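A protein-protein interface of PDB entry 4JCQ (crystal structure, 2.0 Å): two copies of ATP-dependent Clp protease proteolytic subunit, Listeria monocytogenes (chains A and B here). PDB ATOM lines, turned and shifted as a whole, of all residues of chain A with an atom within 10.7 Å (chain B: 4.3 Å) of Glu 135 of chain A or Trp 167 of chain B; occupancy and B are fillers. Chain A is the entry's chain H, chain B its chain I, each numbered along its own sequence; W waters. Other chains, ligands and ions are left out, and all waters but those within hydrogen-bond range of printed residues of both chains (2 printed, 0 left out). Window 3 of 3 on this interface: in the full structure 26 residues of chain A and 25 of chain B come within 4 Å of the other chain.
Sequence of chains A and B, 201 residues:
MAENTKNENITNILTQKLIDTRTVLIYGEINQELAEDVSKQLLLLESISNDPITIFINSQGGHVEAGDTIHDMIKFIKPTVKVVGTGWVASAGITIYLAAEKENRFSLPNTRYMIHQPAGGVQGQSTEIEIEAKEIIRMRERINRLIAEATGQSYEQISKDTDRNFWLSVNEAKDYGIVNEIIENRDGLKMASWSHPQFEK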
ATOM      1  N   GLN A  32       0.895  19.012 -23.760  1.00  0.00           N
ATOM      2  CA  GLN A  32      -0.277  19.795 -23.359  1.00  0.00           C
ATOM      3  C   GLN A  32      -0.019  21.306 -23.390  1.00  0.00           C
ATOM      4  O   GLN A  32      -0.916  22.088 -23.717  1.00  0.00           O
ATOM      5  CB  GLN A  32      -0.792  19.341 -21.986  1.00  0.00           C
ATOM      6  CG  GLN A  32      -1.598  18.047 -22.038  1.00  0.00           C
ATOM      7  CD  GLN A  32      -1.873  17.448 -20.669  1.00  0.00           C
ATOM      8  OE1 GLN A  32      -1.001  17.425 -19.796  1.00  0.00           O
ATOM      9  NE2 GLN A  32      -3.091  16.943 -20.479  1.00  0.00           N
ATOM     10  N   VAL A  64      -0.058  11.581 -27.115  1.00  0.00           N
ATOM     11  CA  VAL A  64      -1.225  11.292 -27.960  1.00  0.00           C
ATOM     12  C   VAL A  64      -2.411  12.237 -27.715  1.00  0.00           C
ATOM     13  O   VAL A  64      -3.013  12.738 -28.668  1.00  0.00           O
ATOM     14  CB  VAL A  64      -1.652   9.797 -27.869  1.00  0.00           C
ATOM     15  CG1 VAL A  64      -1.941   9.380 -26.430  1.00  0.00           C
ATOM     16  CG2 VAL A  64      -2.845   9.504 -28.774  1.00  0.00           C
ATOM     17  N   GLU A  65      -2.723  12.496 -26.446  1.00  0.00           N
ATOM     18  CA  GLU A  65      -3.880  13.317 -26.079  1.00  0.00           C
ATOM     19  C   GLU A  65      -3.722  14.781 -26.504  1.00  0.00           C
ATOM     20  O   GLU A  65      -4.704  15.448 -26.841  1.00  0.00           O
ATOM     21  CB  GLU A  65      -4.188  13.202 -24.576  1.00  0.00           C
ATOM     22  CG  GLU A  65      -3.201  13.892 -23.638  1.00  0.00           C
ATOM     23  CD  GLU A  65      -1.916  13.109 -23.397  1.00  0.00           C
ATOM     24  OE1 GLU A  65      -1.792  11.956 -23.867  1.00  0.00           O
ATOM     25  OE2 GLU A  65      -1.019  13.658 -22.725  1.00  0.00           O
ATOM     26  N   ASP A  68      -4.258  14.726 -30.263  1.00  0.00           N
ATOM     27  CA  ASP A  68      -5.700  14.610 -30.500  1.00  0.00           C
ATOM     28  C   ASP A  68      -6.408  15.961 -30.407  1.00  0.00           C
ATOM     29  O   ASP A  68      -7.262  16.279 -31.237  1.00  0.00           O
ATOM     30  CB  ASP A  68      -6.327  13.614 -29.517  1.00  0.00           C
ATOM     31  CG  ASP A  68      -5.980  12.168 -29.839  1.00  0.00           C
ATOM     32  OD1 ASP A  68      -6.012  11.329 -28.913  1.00  0.00           O
ATOM     33  OD2 ASP A  68      -5.677  11.862 -31.014  1.00  0.00           O
ATOM     34  N   PRO A 118       3.534   5.359 -31.017  1.00  0.00           N
ATOM     35  CA  PRO A 118       3.952   4.689 -29.783  1.00  0.00           C
ATOM     36  C   PRO A 118       2.793   3.909 -29.169  1.00  0.00           C
ATOM     37  O   PRO A 118       1.671   4.415 -29.111  1.00  0.00           O
ATOM     38  CB  PRO A 118       4.365   5.850 -28.871  1.00  0.00           C
ATOM     39  CG  PRO A 118       3.661   7.045 -29.421  1.00  0.00           C
ATOM     40  CD  PRO A 118       3.611   6.826 -30.902  1.00  0.00           C
ATOM     41  N   ALA A 119       3.067   2.681 -28.732  1.00  0.00           N
ATOM     42  CA  ALA A 119       2.031   1.799 -28.195  1.00  0.00           C
ATOM     43  C   ALA A 119       1.356   2.388 -26.953  1.00  0.00           C
ATOM     44  O   ALA A 119       0.127   2.389 -26.847  1.00  0.00           O
ATOM     45  CB  ALA A 119       2.608   0.424 -27.897  1.00  0.00           C
ATOM     46  N   GLY A 120       2.163   2.897 -26.026  1.00  0.00           N
ATOM     47  CA  GLY A 120       1.644   3.534 -24.816  1.00  0.00           C
ATOM     48  C   GLY A 120       1.122   4.939 -25.066  1.00  0.00           C
ATOM     49  O   GLY A 120       0.425   5.507 -24.224  1.00  0.00           O
ATOM     50  N   GLY A 121       1.463   5.495 -26.229  1.00  0.00           N
ATOM     51  CA  GLY A 121       1.083   6.859 -26.595  1.00  0.00           C
ATOM     52  C   GLY A 121       2.041   7.907 -26.056  1.00  0.00           C
ATOM     53  O   GLY A 121       1.754   9.105 -26.129  1.00  0.00           O
ATOM     54  N   ILE A 131      -1.828   2.405 -18.427  1.00  0.00           N
ATOM     55  CA  ILE A 131      -2.779   2.045 -19.478  1.00  0.00           C
ATOM     56  C   ILE A 131      -2.730   0.540 -19.770  1.00  0.00           C
ATOM     57  O   ILE A 131      -1.660  -0.026 -20.011  1.00  0.00           O
ATOM     58  CB  ILE A 131      -2.576   2.910 -20.754  1.00  0.00           C
ATOM     59  CG1 ILE A 131      -3.334   4.239 -20.631  1.00  0.00           C
ATOM     60  CG2 ILE A 131      -3.077   2.207 -22.007  1.00  0.00           C
ATOM     61  CD1 ILE A 131      -2.606   5.326 -19.868  1.00  0.00           C
ATOM     62  N   GLU A 132      -3.901  -0.095 -19.727  1.00  0.00           N
ATOM     63  CA  GLU A 132      -4.027  -1.538 -19.937  1.00  0.00           C
ATOM     64  C   GLU A 132      -3.916  -1.910 -21.415  1.00  0.00           C
ATOM     65  O   GLU A 132      -4.056  -1.050 -22.288  1.00  0.00           O
ATOM     66  CB  GLU A 132      -5.353  -2.050 -19.361  1.00  0.00           C
ATOM     67  CG  GLU A 132      -5.597  -1.705 -17.895  1.00  0.00           C
ATOM     68  CD  GLU A 132      -4.586  -2.330 -16.943  1.00  0.00           C
ATOM     69  OE1 GLU A 132      -4.272  -1.692 -15.918  1.00  0.00           O
ATOM     70  OE2 GLU A 132      -4.104  -3.453 -17.209  1.00  0.00           O
ATOM     71  N   ALA A 133      -3.670  -3.192 -21.683  1.00  0.00           N
ATOM     72  CA  ALA A 133      -3.524  -3.696 -23.050  1.00  0.00           C
ATOM     73  C   ALA A 133      -4.767  -3.452 -23.905  1.00  0.00           C
ATOM     74  O   ALA A 133      -4.652  -3.138 -25.089  1.00  0.00           O
ATOM     75  CB  ALA A 133      -3.163  -5.176 -23.041  1.00  0.00           C
ATOM     76  N   LYS A 134      -5.948  -3.587 -23.298  1.00  0.00           N
ATOM     77  CA  LYS A 134      -7.217  -3.350 -23.994  1.00  0.00           C
ATOM     78  C   LYS A 134      -7.321  -1.912 -24.511  1.00  0.00           C
ATOM     79  O   LYS A 134      -7.889  -1.665 -25.576  1.00  0.00           O
ATOM     80  CB  LYS A 134      -8.416  -3.700 -23.095  1.00  0.00           C
ATOM     81  CG  LYS A 134      -8.716  -2.701 -21.984  1.00  0.00           C
ATOM     82  CD  LYS A 134      -9.993  -3.050 -21.229  1.00  0.00           C
ATOM     83  CE  LYS A 134      -9.708  -3.669 -19.867  1.00  0.00           C
ATOM     84  NZ  LYS A 134      -9.095  -5.022 -19.939  1.00  0.00           N
ATOM     85  N   GLU A 135      -6.755  -0.975 -23.754  1.00  0.00           N
ATOM     86  CA  GLU A 135      -6.783   0.437 -24.114  1.00  0.00           C
ATOM     87  C   GLU A 135      -5.719   0.783 -25.157  1.00  0.00           C
ATOM     88  O   GLU A 135      -5.937   1.653 -26.004  1.00  0.00           O
ATOM     89  CB  GLU A 135      -6.647   1.308 -22.860  1.00  0.00           C
ATOM     90  CG  GLU A 135      -6.917   2.793 -23.070  1.00  0.00           C
ATOM     91  CD  GLU A 135      -8.286   3.101 -23.665  1.00  0.00           C
ATOM     92  OE1 GLU A 135      -9.232   2.296 -23.508  1.00  0.00           O
ATOM     93  OE2 GLU A 135      -8.420   4.172 -24.288  1.00  0.00           O
ATOM     94  N   ILE A 136      -4.576   0.099 -25.094  1.00  0.00           N
ATOM     95  CA  ILE A 136      -3.538   0.213 -26.122  1.00  0.00           C
ATOM     96  C   ILE A 136      -4.106  -0.183 -27.488  1.00  0.00           C
ATOM     97  O   ILE A 136      -3.880   0.507 -28.484  1.00  0.00           O
ATOM     98  CB  ILE A 136      -2.289  -0.638 -25.781  1.00  0.00           C
ATOM     99  CG1 ILE A 136      -1.549  -0.040 -24.582  1.00  0.00           C
ATOM    100  CG2 ILE A 136      -1.352  -0.747 -26.981  1.00  0.00           C
ATOM    101  CD1 ILE A 136      -0.458  -0.925 -24.008  1.00  0.00           C
ATOM    102  N   ILE A 137      -4.853  -1.287 -27.515  1.00  0.00           N
ATOM    103  CA  ILE A 137      -5.499  -1.778 -28.735  1.00  0.00           C
ATOM    104  C   ILE A 137      -6.532  -0.780 -29.262  1.00  0.00           C
ATOM    105  O   ILE A 137      -6.532  -0.456 -30.450  1.00  0.00           O
ATOM    106  CB  ILE A 137      -6.133  -3.179 -28.521  1.00  0.00           C
ATOM    107  CG1 ILE A 137      -5.057  -4.223 -28.183  1.00  0.00           C
ATOM    108  CG2 ILE A 137      -6.957  -3.615 -29.729  1.00  0.00           C
ATOM    109  CD1 ILE A 137      -3.907  -4.303 -29.171  1.00  0.00           C
ATOM    110  N   ARG A 138      -7.392  -0.290 -28.370  1.00  0.00           N
ATOM    111  CA  ARG A 138      -8.416   0.700 -28.722  1.00  0.00           C
ATOM    112  C   ARG A 138      -7.811   1.976 -29.299  1.00  0.00           C
ATOM    113  O   ARG A 138      -8.277   2.480 -30.321  1.00  0.00           O
ATOM    114  CB  ARG A 138      -9.269   1.045 -27.501  1.00  0.00           C
ATOM    115  CG  ARG A 138     -10.433   0.107 -27.261  1.00  0.00           C
ATOM    116  CD  ARG A 138     -11.339   0.668 -26.182  1.00  0.00           C
ATOM    117  NE  ARG A 138     -12.688   0.120 -26.267  1.00  0.00           N
ATOM    118  CZ  ARG A 138     -13.722   0.549 -25.549  1.00  0.00           C
ATOM    119  NH1 ARG A 138     -13.572   1.541 -24.679  1.00  0.00           N
ATOM    120  NH2 ARG A 138     -14.910  -0.018 -25.703  1.00  0.00           N
ATOM    121  N   MET A 139      -6.778   2.488 -28.631  1.00  0.00           N
ATOM    122  CA  MET A 139      -6.049   3.678 -29.076  1.00  0.00           C
ATOM    123  C   MET A 139      -5.475   3.470 -30.474  1.00  0.00           C
ATOM    124  O   MET A 139      -5.640   4.321 -31.348  1.00  0.00           O
ATOM    125  CB  MET A 139      -4.922   4.007 -28.090  1.00  0.00           C
ATOM    126  CG  MET A 139      -4.146   5.280 -28.397  1.00  0.00           C
ATOM    127  SD  MET A 139      -2.660   5.468 -27.385  1.00  0.00           S
ATOM    128  CE  MET A 139      -3.360   5.763 -25.763  1.00  0.00           C
ATOM    129  N   ARG A 140      -4.816   2.329 -30.673  1.00  0.00           N
ATOM    130  CA  ARG A 140      -4.218   1.991 -31.962  1.00  0.00           C
ATOM    131  C   ARG A 140      -5.256   1.905 -33.078  1.00  0.00           C
ATOM    132  O   ARG A 140      -5.042   2.444 -34.163  1.00  0.00           O
ATOM    133  CB  ARG A 140      -3.411   0.688 -31.864  1.00  0.00           C
ATOM    134  CG  ARG A 140      -2.700   0.281 -33.152  1.00  0.00           C
ATOM    135  CD  ARG A 140      -1.772   1.377 -33.675  1.00  0.00           C
ATOM    136  NE  ARG A 140      -0.706   1.697 -32.727  1.00  0.00           N
ATOM    137  CZ  ARG A 140       0.455   1.051 -32.647  1.00  0.00           C
ATOM    138  NH1 ARG A 140       1.350   1.419 -31.742  1.00  0.00           N
ATOM    139  NH2 ARG A 140       0.722   0.041 -33.464  1.00  0.00           N
ATOM    140  N   GLU A 141      -6.376   1.235 -32.803  1.00  0.00           N
ATOM    141  CA  GLU A 141      -7.470   1.115 -33.769  1.00  0.00           C
ATOM    142  C   GLU A 141      -8.025   2.485 -34.171  1.00  0.00           C
ATOM    143  O   GLU A 141      -8.262   2.739 -35.353  1.00  0.00           O
ATOM    144  CB  GLU A 141      -8.588   0.220 -33.221  1.00  0.00           C
ATOM    145  CG  GLU A 141      -8.220  -1.256 -33.145  1.00  0.00           C
ATOM    146  CD  GLU A 141      -9.285  -2.114 -32.481  1.00  0.00           C
ATOM    147  OE1 GLU A 141      -9.065  -3.338 -32.364  1.00  0.00           O
ATOM    148  OE2 GLU A 141     -10.338  -1.575 -32.074  1.00  0.00           O
ATOM    149  N   ARG A 142      -8.212   3.360 -33.184  1.00  0.00           N
ATOM    150  CA  ARG A 142      -8.711   4.718 -33.418  1.00  0.00           C
ATOM    151  C   ARG A 142      -7.769   5.520 -34.322  1.00  0.00           C
ATOM    152  O   ARG A 142      -8.205   6.127 -35.299  1.00  0.00           O
ATOM    153  CB  ARG A 142      -8.933   5.445 -32.085  1.00  0.00           C
ATOM    154  CG  ARG A 142      -9.475   6.863 -32.217  1.00  0.00           C
ATOM    155  CD  ARG A 142      -9.675   7.535 -30.864  1.00  0.00           C
ATOM    156  NE  ARG A 142      -8.437   7.622 -30.081  1.00  0.00           N
ATOM    157  CZ  ARG A 142      -7.522   8.582 -30.205  1.00  0.00           C
ATOM    158  NH1 ARG A 142      -6.436   8.566 -29.444  1.00  0.00           N
ATOM    159  NH2 ARG A 142      -7.680   9.559 -31.088  1.00  0.00           N
ATOM    160  N   ILE A 143      -6.478   5.506 -33.997  1.00  0.00           N
ATOM    161  CA  ILE A 143      -5.483   6.249 -34.771  1.00  0.00           C
ATOM    162  C   ILE A 143      -5.285   5.640 -36.166  1.00  0.00           C
ATOM    163  O   ILE A 143      -5.134   6.378 -37.146  1.00  0.00           O
ATOM    164  CB  ILE A 143      -4.143   6.380 -34.008  1.00  0.00           C
ATOM    165  CG1 ILE A 143      -4.367   7.126 -32.685  1.00  0.00           C
ATOM    166  CG2 ILE A 143      -3.109   7.122 -34.850  1.00  0.00           C
ATOM    167  CD1 ILE A 143      -3.250   6.967 -31.674  1.00  0.00           C
ATOM    168  N   ASN A 144      -5.307   4.309 -36.251  1.00  0.00           N
ATOM    169  CA  ASN A 144      -5.224   3.611 -37.538  1.00  0.00           C
ATOM    170  C   ASN A 144      -6.341   4.018 -38.498  1.00  0.00           C
ATOM    171  O   ASN A 144      -6.086   4.271 -39.676  1.00  0.00           O
ATOM    172  CB  ASN A 144      -5.227   2.085 -37.353  1.00  0.00           C
ATOM    173  CG  ASN A 144      -3.888   1.540 -36.881  1.00  0.00           C
ATOM    174  OD1 ASN A 144      -2.862   2.220 -36.943  1.00  0.00           O
ATOM    175  ND2 ASN A 144      -3.896   0.299 -36.406  1.00  0.00           N
ATOM    176  N   ARG A 145      -7.572   4.079 -37.986  1.00  0.00           N
ATOM    177  CA  ARG A 145      -8.731   4.498 -38.780  1.00  0.00           C
ATOM    178  C   ARG A 145      -8.611   5.956 -39.221  1.00  0.00           C
ATOM    179  O   ARG A 145      -8.933   6.297 -40.358  1.00  0.00           O
ATOM    180  CB  ARG A 145     -10.035   4.283 -38.005  1.00  0.00           C
ATOM    181  CG  ARG A 145     -10.459   2.827 -37.888  1.00  0.00           C
ATOM    182  CD  ARG A 145     -11.855   2.699 -37.298  1.00  0.00           C
ATOM    183  NE  ARG A 145     -12.250   1.298 -37.144  1.00  0.00           N
ATOM    184  CZ  ARG A 145     -12.151   0.603 -36.013  1.00  0.00           C
ATOM    185  NH1 ARG A 145     -11.671   1.169 -34.910  1.00  0.00           N
ATOM    186  NH2 ARG A 145     -12.536  -0.665 -35.982  1.00  0.00           N
ATOM    187  N   TRP B  88      -8.126  13.973 -23.393  1.00  0.00           N
ATOM    188  CA  TRP B  88      -8.668  13.158 -22.304  1.00  0.00           C
ATOM    189  C   TRP B  88      -9.254  13.975 -21.186  1.00  0.00           C
ATOM    190  O   TRP B  88      -8.867  15.124 -20.969  1.00  0.00           O
ATOM    191  CB  TRP B  88      -7.668  12.112 -21.783  1.00  0.00           C
ATOM    192  CG  TRP B  88      -6.349  12.623 -21.239  1.00  0.00           C
ATOM    193  CD1 TRP B  88      -5.976  13.941 -20.969  1.00  0.00           C
ATOM    194  CD2 TRP B  88      -5.187  11.814 -20.838  1.00  0.00           C
ATOM    195  NE1 TRP B  88      -4.699  13.996 -20.468  1.00  0.00           N
ATOM    196  CE2 TRP B  88      -4.171  12.758 -20.359  1.00  0.00           C
ATOM    197  CE3 TRP B  88      -4.897  10.452 -20.835  1.00  0.00           C
ATOM    198  CZ2 TRP B  88      -2.928  12.335 -19.906  1.00  0.00           C
ATOM    199  CZ3 TRP B  88      -3.640  10.038 -20.374  1.00  0.00           C
ATOM    200  CH2 TRP B  88      -2.681  10.958 -19.922  1.00  0.00           C
ATOM    201  N   ALA B  90     -10.219  13.038 -17.189  1.00  0.00           N
ATOM    202  CA  ALA B  90     -10.167  11.992 -16.173  1.00  0.00           C
ATOM    203  C   ALA B  90     -10.123  12.536 -14.753  1.00  0.00           C
ATOM    204  O   ALA B  90      -9.596  13.624 -14.511  1.00  0.00           O
ATOM    205  CB  ALA B  90      -8.981  11.071 -16.422  1.00  0.00           C
ATOM    206  N   ARG B 112     -10.999  10.530 -24.754  1.00  0.00           N
ATOM    207  CA  ARG B 112     -11.389   9.434 -23.866  1.00  0.00           C
ATOM    208  C   ARG B 112     -11.658   9.943 -22.449  1.00  0.00           C
ATOM    209  O   ARG B 112     -11.114  10.968 -22.034  1.00  0.00           O
ATOM    210  CB  ARG B 112     -10.355   8.297 -23.878  1.00  0.00           C
ATOM    211  CG  ARG B 112      -8.903   8.730 -23.767  1.00  0.00           C
ATOM    212  CD  ARG B 112      -7.994   7.516 -23.660  1.00  0.00           C
ATOM    213  NE  ARG B 112      -6.588   7.889 -23.521  1.00  0.00           N
ATOM    214  CZ  ARG B 112      -5.648   7.099 -23.009  1.00  0.00           C
ATOM    215  NH1 ARG B 112      -4.395   7.525 -22.923  1.00  0.00           N
ATOM    216  NH2 ARG B 112      -5.956   5.886 -22.570  1.00  0.00           N
ATOM    217  N   TYR B 113     -12.510   9.222 -21.724  1.00  0.00           N
ATOM    218  CA  TYR B 113     -12.999   9.652 -20.415  1.00  0.00           C
ATOM    219  C   TYR B 113     -12.802   8.557 -19.372  1.00  0.00           C
ATOM    220  O   TYR B 113     -12.970   7.375 -19.671  1.00  0.00           O
ATOM    221  CB  TYR B 113     -14.488  10.022 -20.503  1.00  0.00           C
ATOM    222  CG  TYR B 113     -14.773  11.251 -21.342  1.00  0.00           C
ATOM    223  CD1 TYR B 113     -15.017  12.485 -20.741  1.00  0.00           C
ATOM    224  CD2 TYR B 113     -14.793  11.182 -22.737  1.00  0.00           C
ATOM    225  CE1 TYR B 113     -15.277  13.614 -21.501  1.00  0.00           C
ATOM    226  CE2 TYR B 113     -15.047  12.305 -23.506  1.00  0.00           C
ATOM    227  CZ  TYR B 113     -15.282  13.518 -22.883  1.00  0.00           C
ATOM    228  OH  TYR B 113     -15.536  14.636 -23.641  1.00  0.00           O
ATOM    229  N   MET B 114     -12.441   8.953 -18.153  1.00  0.00           N
ATOM    230  CA  MET B 114     -12.301   8.008 -17.042  1.00  0.00           C
ATOM    231  C   MET B 114     -12.757   8.649 -15.735  1.00  0.00           C
ATOM    232  O   MET B 114     -12.241   9.693 -15.338  1.00  0.00           O
ATOM    233  CB  MET B 114     -10.855   7.505 -16.926  1.00  0.00           C
ATOM    234  CG  MET B 114     -10.644   6.459 -15.837  1.00  0.00           C
ATOM    235  SD  MET B 114      -8.976   5.769 -15.772  1.00  0.00           S
ATOM    236  CE  MET B 114      -8.034   7.172 -15.181  1.00  0.00           C
ATOM    237  N   PHE B 166     -10.907   2.273 -15.785  1.00  0.00           N
ATOM    238  CA  PHE B 166     -11.317   1.932 -17.140  1.00  0.00           C
ATOM    239  C   PHE B 166     -11.653   3.167 -17.966  1.00  0.00           C
ATOM    240  O   PHE B 166     -12.356   4.075 -17.512  1.00  0.00           O
ATOM    241  CB  PHE B 166     -12.465   0.911 -17.140  1.00  0.00           C
ATOM    242  CG  PHE B 166     -13.800   1.488 -16.771  1.00  0.00           C
ATOM    243  CD1 PHE B 166     -14.769   1.701 -17.746  1.00  0.00           C
ATOM    244  CD2 PHE B 166     -14.094   1.815 -15.453  1.00  0.00           C
ATOM    245  CE1 PHE B 166     -16.005   2.231 -17.412  1.00  0.00           C
ATOM    246  CE2 PHE B 166     -15.325   2.349 -15.114  1.00  0.00           C
ATOM    247  CZ  PHE B 166     -16.284   2.557 -16.095  1.00  0.00           C
ATOM    248  N   TRP B 167     -11.127   3.188 -19.183  1.00  0.00           N
ATOM    249  CA  TRP B 167     -11.329   4.298 -20.094  1.00  0.00           C
ATOM    250  C   TRP B 167     -12.549   4.103 -20.939  1.00  0.00           C
ATOM    251  O   TRP B 167     -12.782   3.021 -21.482  1.00  0.00           O
ATOM    252  CB  TRP B 167     -10.098   4.490 -20.965  1.00  0.00           C
ATOM    253  CG  TRP B 167      -8.942   5.102 -20.216  1.00  0.00           C
ATOM    254  CD1 TRP B 167      -7.878   4.443 -19.604  1.00  0.00           C
ATOM    255  CD2 TRP B 167      -8.707   6.528 -19.958  1.00  0.00           C
ATOM    256  NE1 TRP B 167      -7.022   5.338 -19.013  1.00  0.00           N
ATOM    257  CE2 TRP B 167      -7.459   6.605 -19.187  1.00  0.00           C
ATOM    258  CE3 TRP B 167      -9.374   7.705 -20.280  1.00  0.00           C
ATOM    259  CZ2 TRP B 167      -6.927   7.816 -18.769  1.00  0.00           C
ATOM    260  CZ3 TRP B 167      -8.825   8.921 -19.854  1.00  0.00           C
ATOM    261  CH2 TRP B 167      -7.631   8.971 -19.117  1.00  0.00           C
ATOM    262  N   LEU B 168     -13.344   5.161 -21.043  1.00  0.00           N
ATOM    263  CA  LEU B 168     -14.507   5.177 -21.913  1.00  0.00           C
ATOM    264  C   LEU B 168     -14.173   5.921 -23.194  1.00  0.00           C
ATOM    265  O   LEU B 168     -13.571   6.998 -23.155  1.00  0.00           O
ATOM    266  CB  LEU B 168     -15.692   5.855 -21.216  1.00  0.00           C
ATOM    267  CG  LEU B 168     -16.268   5.212 -19.952  1.00  0.00           C
ATOM    268  CD1 LEU B 168     -17.074   6.234 -19.166  1.00  0.00           C
ATOM    269  CD2 LEU B 168     -17.117   3.993 -20.285  1.00  0.00           C
ATOM    270  N   SER B 169     -14.559   5.342 -24.327  1.00  0.00           N
ATOM    271  CA  SER B 169     -14.496   6.042 -25.605  1.00  0.00           C
ATOM    272  C   SER B 169     -15.504   7.188 -25.582  1.00  0.00           C
ATOM    273  O   SER B 169     -16.356   7.248 -24.693  1.00  0.00           O
ATOM    274  CB  SER B 169     -14.805   5.088 -26.759  1.00  0.00           C
ATOM    275  OG  SER B 169     -16.172   4.717 -26.757  1.00  0.00           O
ATOM    276  N   GLU B 172     -18.997   5.800 -25.636  1.00  0.00           N
ATOM    277  CA  GLU B 172     -19.328   5.183 -24.351  1.00  0.00           C
ATOM    278  C   GLU B 172     -19.599   6.234 -23.277  1.00  0.00           C
ATOM    279  O   GLU B 172     -20.486   6.057 -22.444  1.00  0.00           O
ATOM    280  CB  GLU B 172     -18.214   4.240 -23.896  1.00  0.00           C
ATOM    281  CG  GLU B 172     -18.116   2.950 -24.695  1.00  0.00           C
ATOM    282  CD  GLU B 172     -16.935   2.091 -24.285  1.00  0.00           C
ATOM    283  OE1 GLU B 172     -15.880   2.650 -23.915  1.00  0.00           O
ATOM    284  OE2 GLU B 172     -17.060   0.851 -24.341  1.00  0.00           O
HETATM  285  O   HOH W   1      -3.410   9.778 -23.569  1.00  0.00           O
HETATM  286  O   HOH W   2      -6.394   4.875 -25.595  1.00  0.00           O
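No position is printed for both chains.
Water W2 bridges OE2 of Glu 135 of chain A (2.5 Å) and NH2 of Arg 112 of chain B (3.2 Å).
Water W1 lies within hydrogen-bond range of NH1 of Arg 112 of chain B (2.5 Å) and OE1 of Glu 65 of chain A (2.7 Å).
Glu 135 of chain A touches just these residues of chain B: Arg 112 and Trp 167.
Trp 167 of chain B touches just these residues of chain A: Glu 135 and Arg 138.
Of chain A, only Gln 32 and Glu 65 come within 4 Å of Trp 88 of chain B.
Arg 112 of chain B touches just these residues of chain A: Ile 131, Glu 135 and Met 139.
Phe 166 of chain B touches none of the printed residues of chain A.
Of chain A, only Arg 138 (3.9 Å) comes within 4 Å of Ser 169 of chain B.
Printed residues of chain B within 4 Å of Ile 131 of chain A: Arg 112.
Printed residues of chain A within 4 Å of Glu 172 of chain B: Arg 138 (2.7 Å).
Printed residues of chain B within 4 Å of Arg 138 of chain A: Trp 167, Ser 169 and Glu 172.
Ile 137 of chain A touches none of the printed residues of chain B.
The nearest printed residue of chain B that does not touch Glu 135 of chain A is Leu 168 of chain B (5.6 Å).
The nearest printed residue of chain B that does not touch Arg 138 of chain A is Leu 168 of chain B (4.7 Å).
Of the 10 printed residues of chain B, 5 touch a printed residue of chain A.
Hydrophobic or aromatic side chains of chain B within 4 Å of the printed part of chain A: Trp 88 and Trp 167.
Printed residues of chain A that touch a printed residue of chain B: Gln 32, Glu 65, Ile 131, Glu 135, Arg 138 and Met 139.
Hydrophobic or aromatic side chains of chain A within 4 Å of the printed part of chain B: Ile 131 and Met 139.
Glu 65 of chain A touches Trp 88 of chain B.
NH2 of Arg 112 of chain B touches CG1 of Ile 131 of chain A, at 3.7 Å.
Glu 135 of chain A touches Trp 167 of chain B (OE1 to CB, 3.5 Å).
NH1 of Arg 138 of chain A touches O of Trp 167 of chain B, 3.6 Å away.
N of Ser 169 of chain B touches NH1 of Arg 138 of chain A, at 3.9 Å.
Met 139 of chain A touches Arg 112 of chain B (CE to NH1, 3.5 Å).
The guanidinium group (NH1) of Arg 138 of chain A is in salt-bridge range of the side-chain carboxylate (OE1) of Glu 172 of chain B (2.7 Å).
The side-chain carboxylate (OE2) of Glu 135 of chain A lies within salt-bridge range of the guanidinium group (NH2) of Arg 112 of chain B (3.5 Å).
The indole nitrogen (NE1) of Trp 88 of chain B lies close to the side-chain amide nitrogen (NE2) of Gln 32 of chain A, 3.4 Å away.
The backbone NH (N) of Ser 169 of chain B lies within hydrogen-bond range of the side-chain carboxylate (OE1) of Glu 172 of chain B (3.0 Å).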
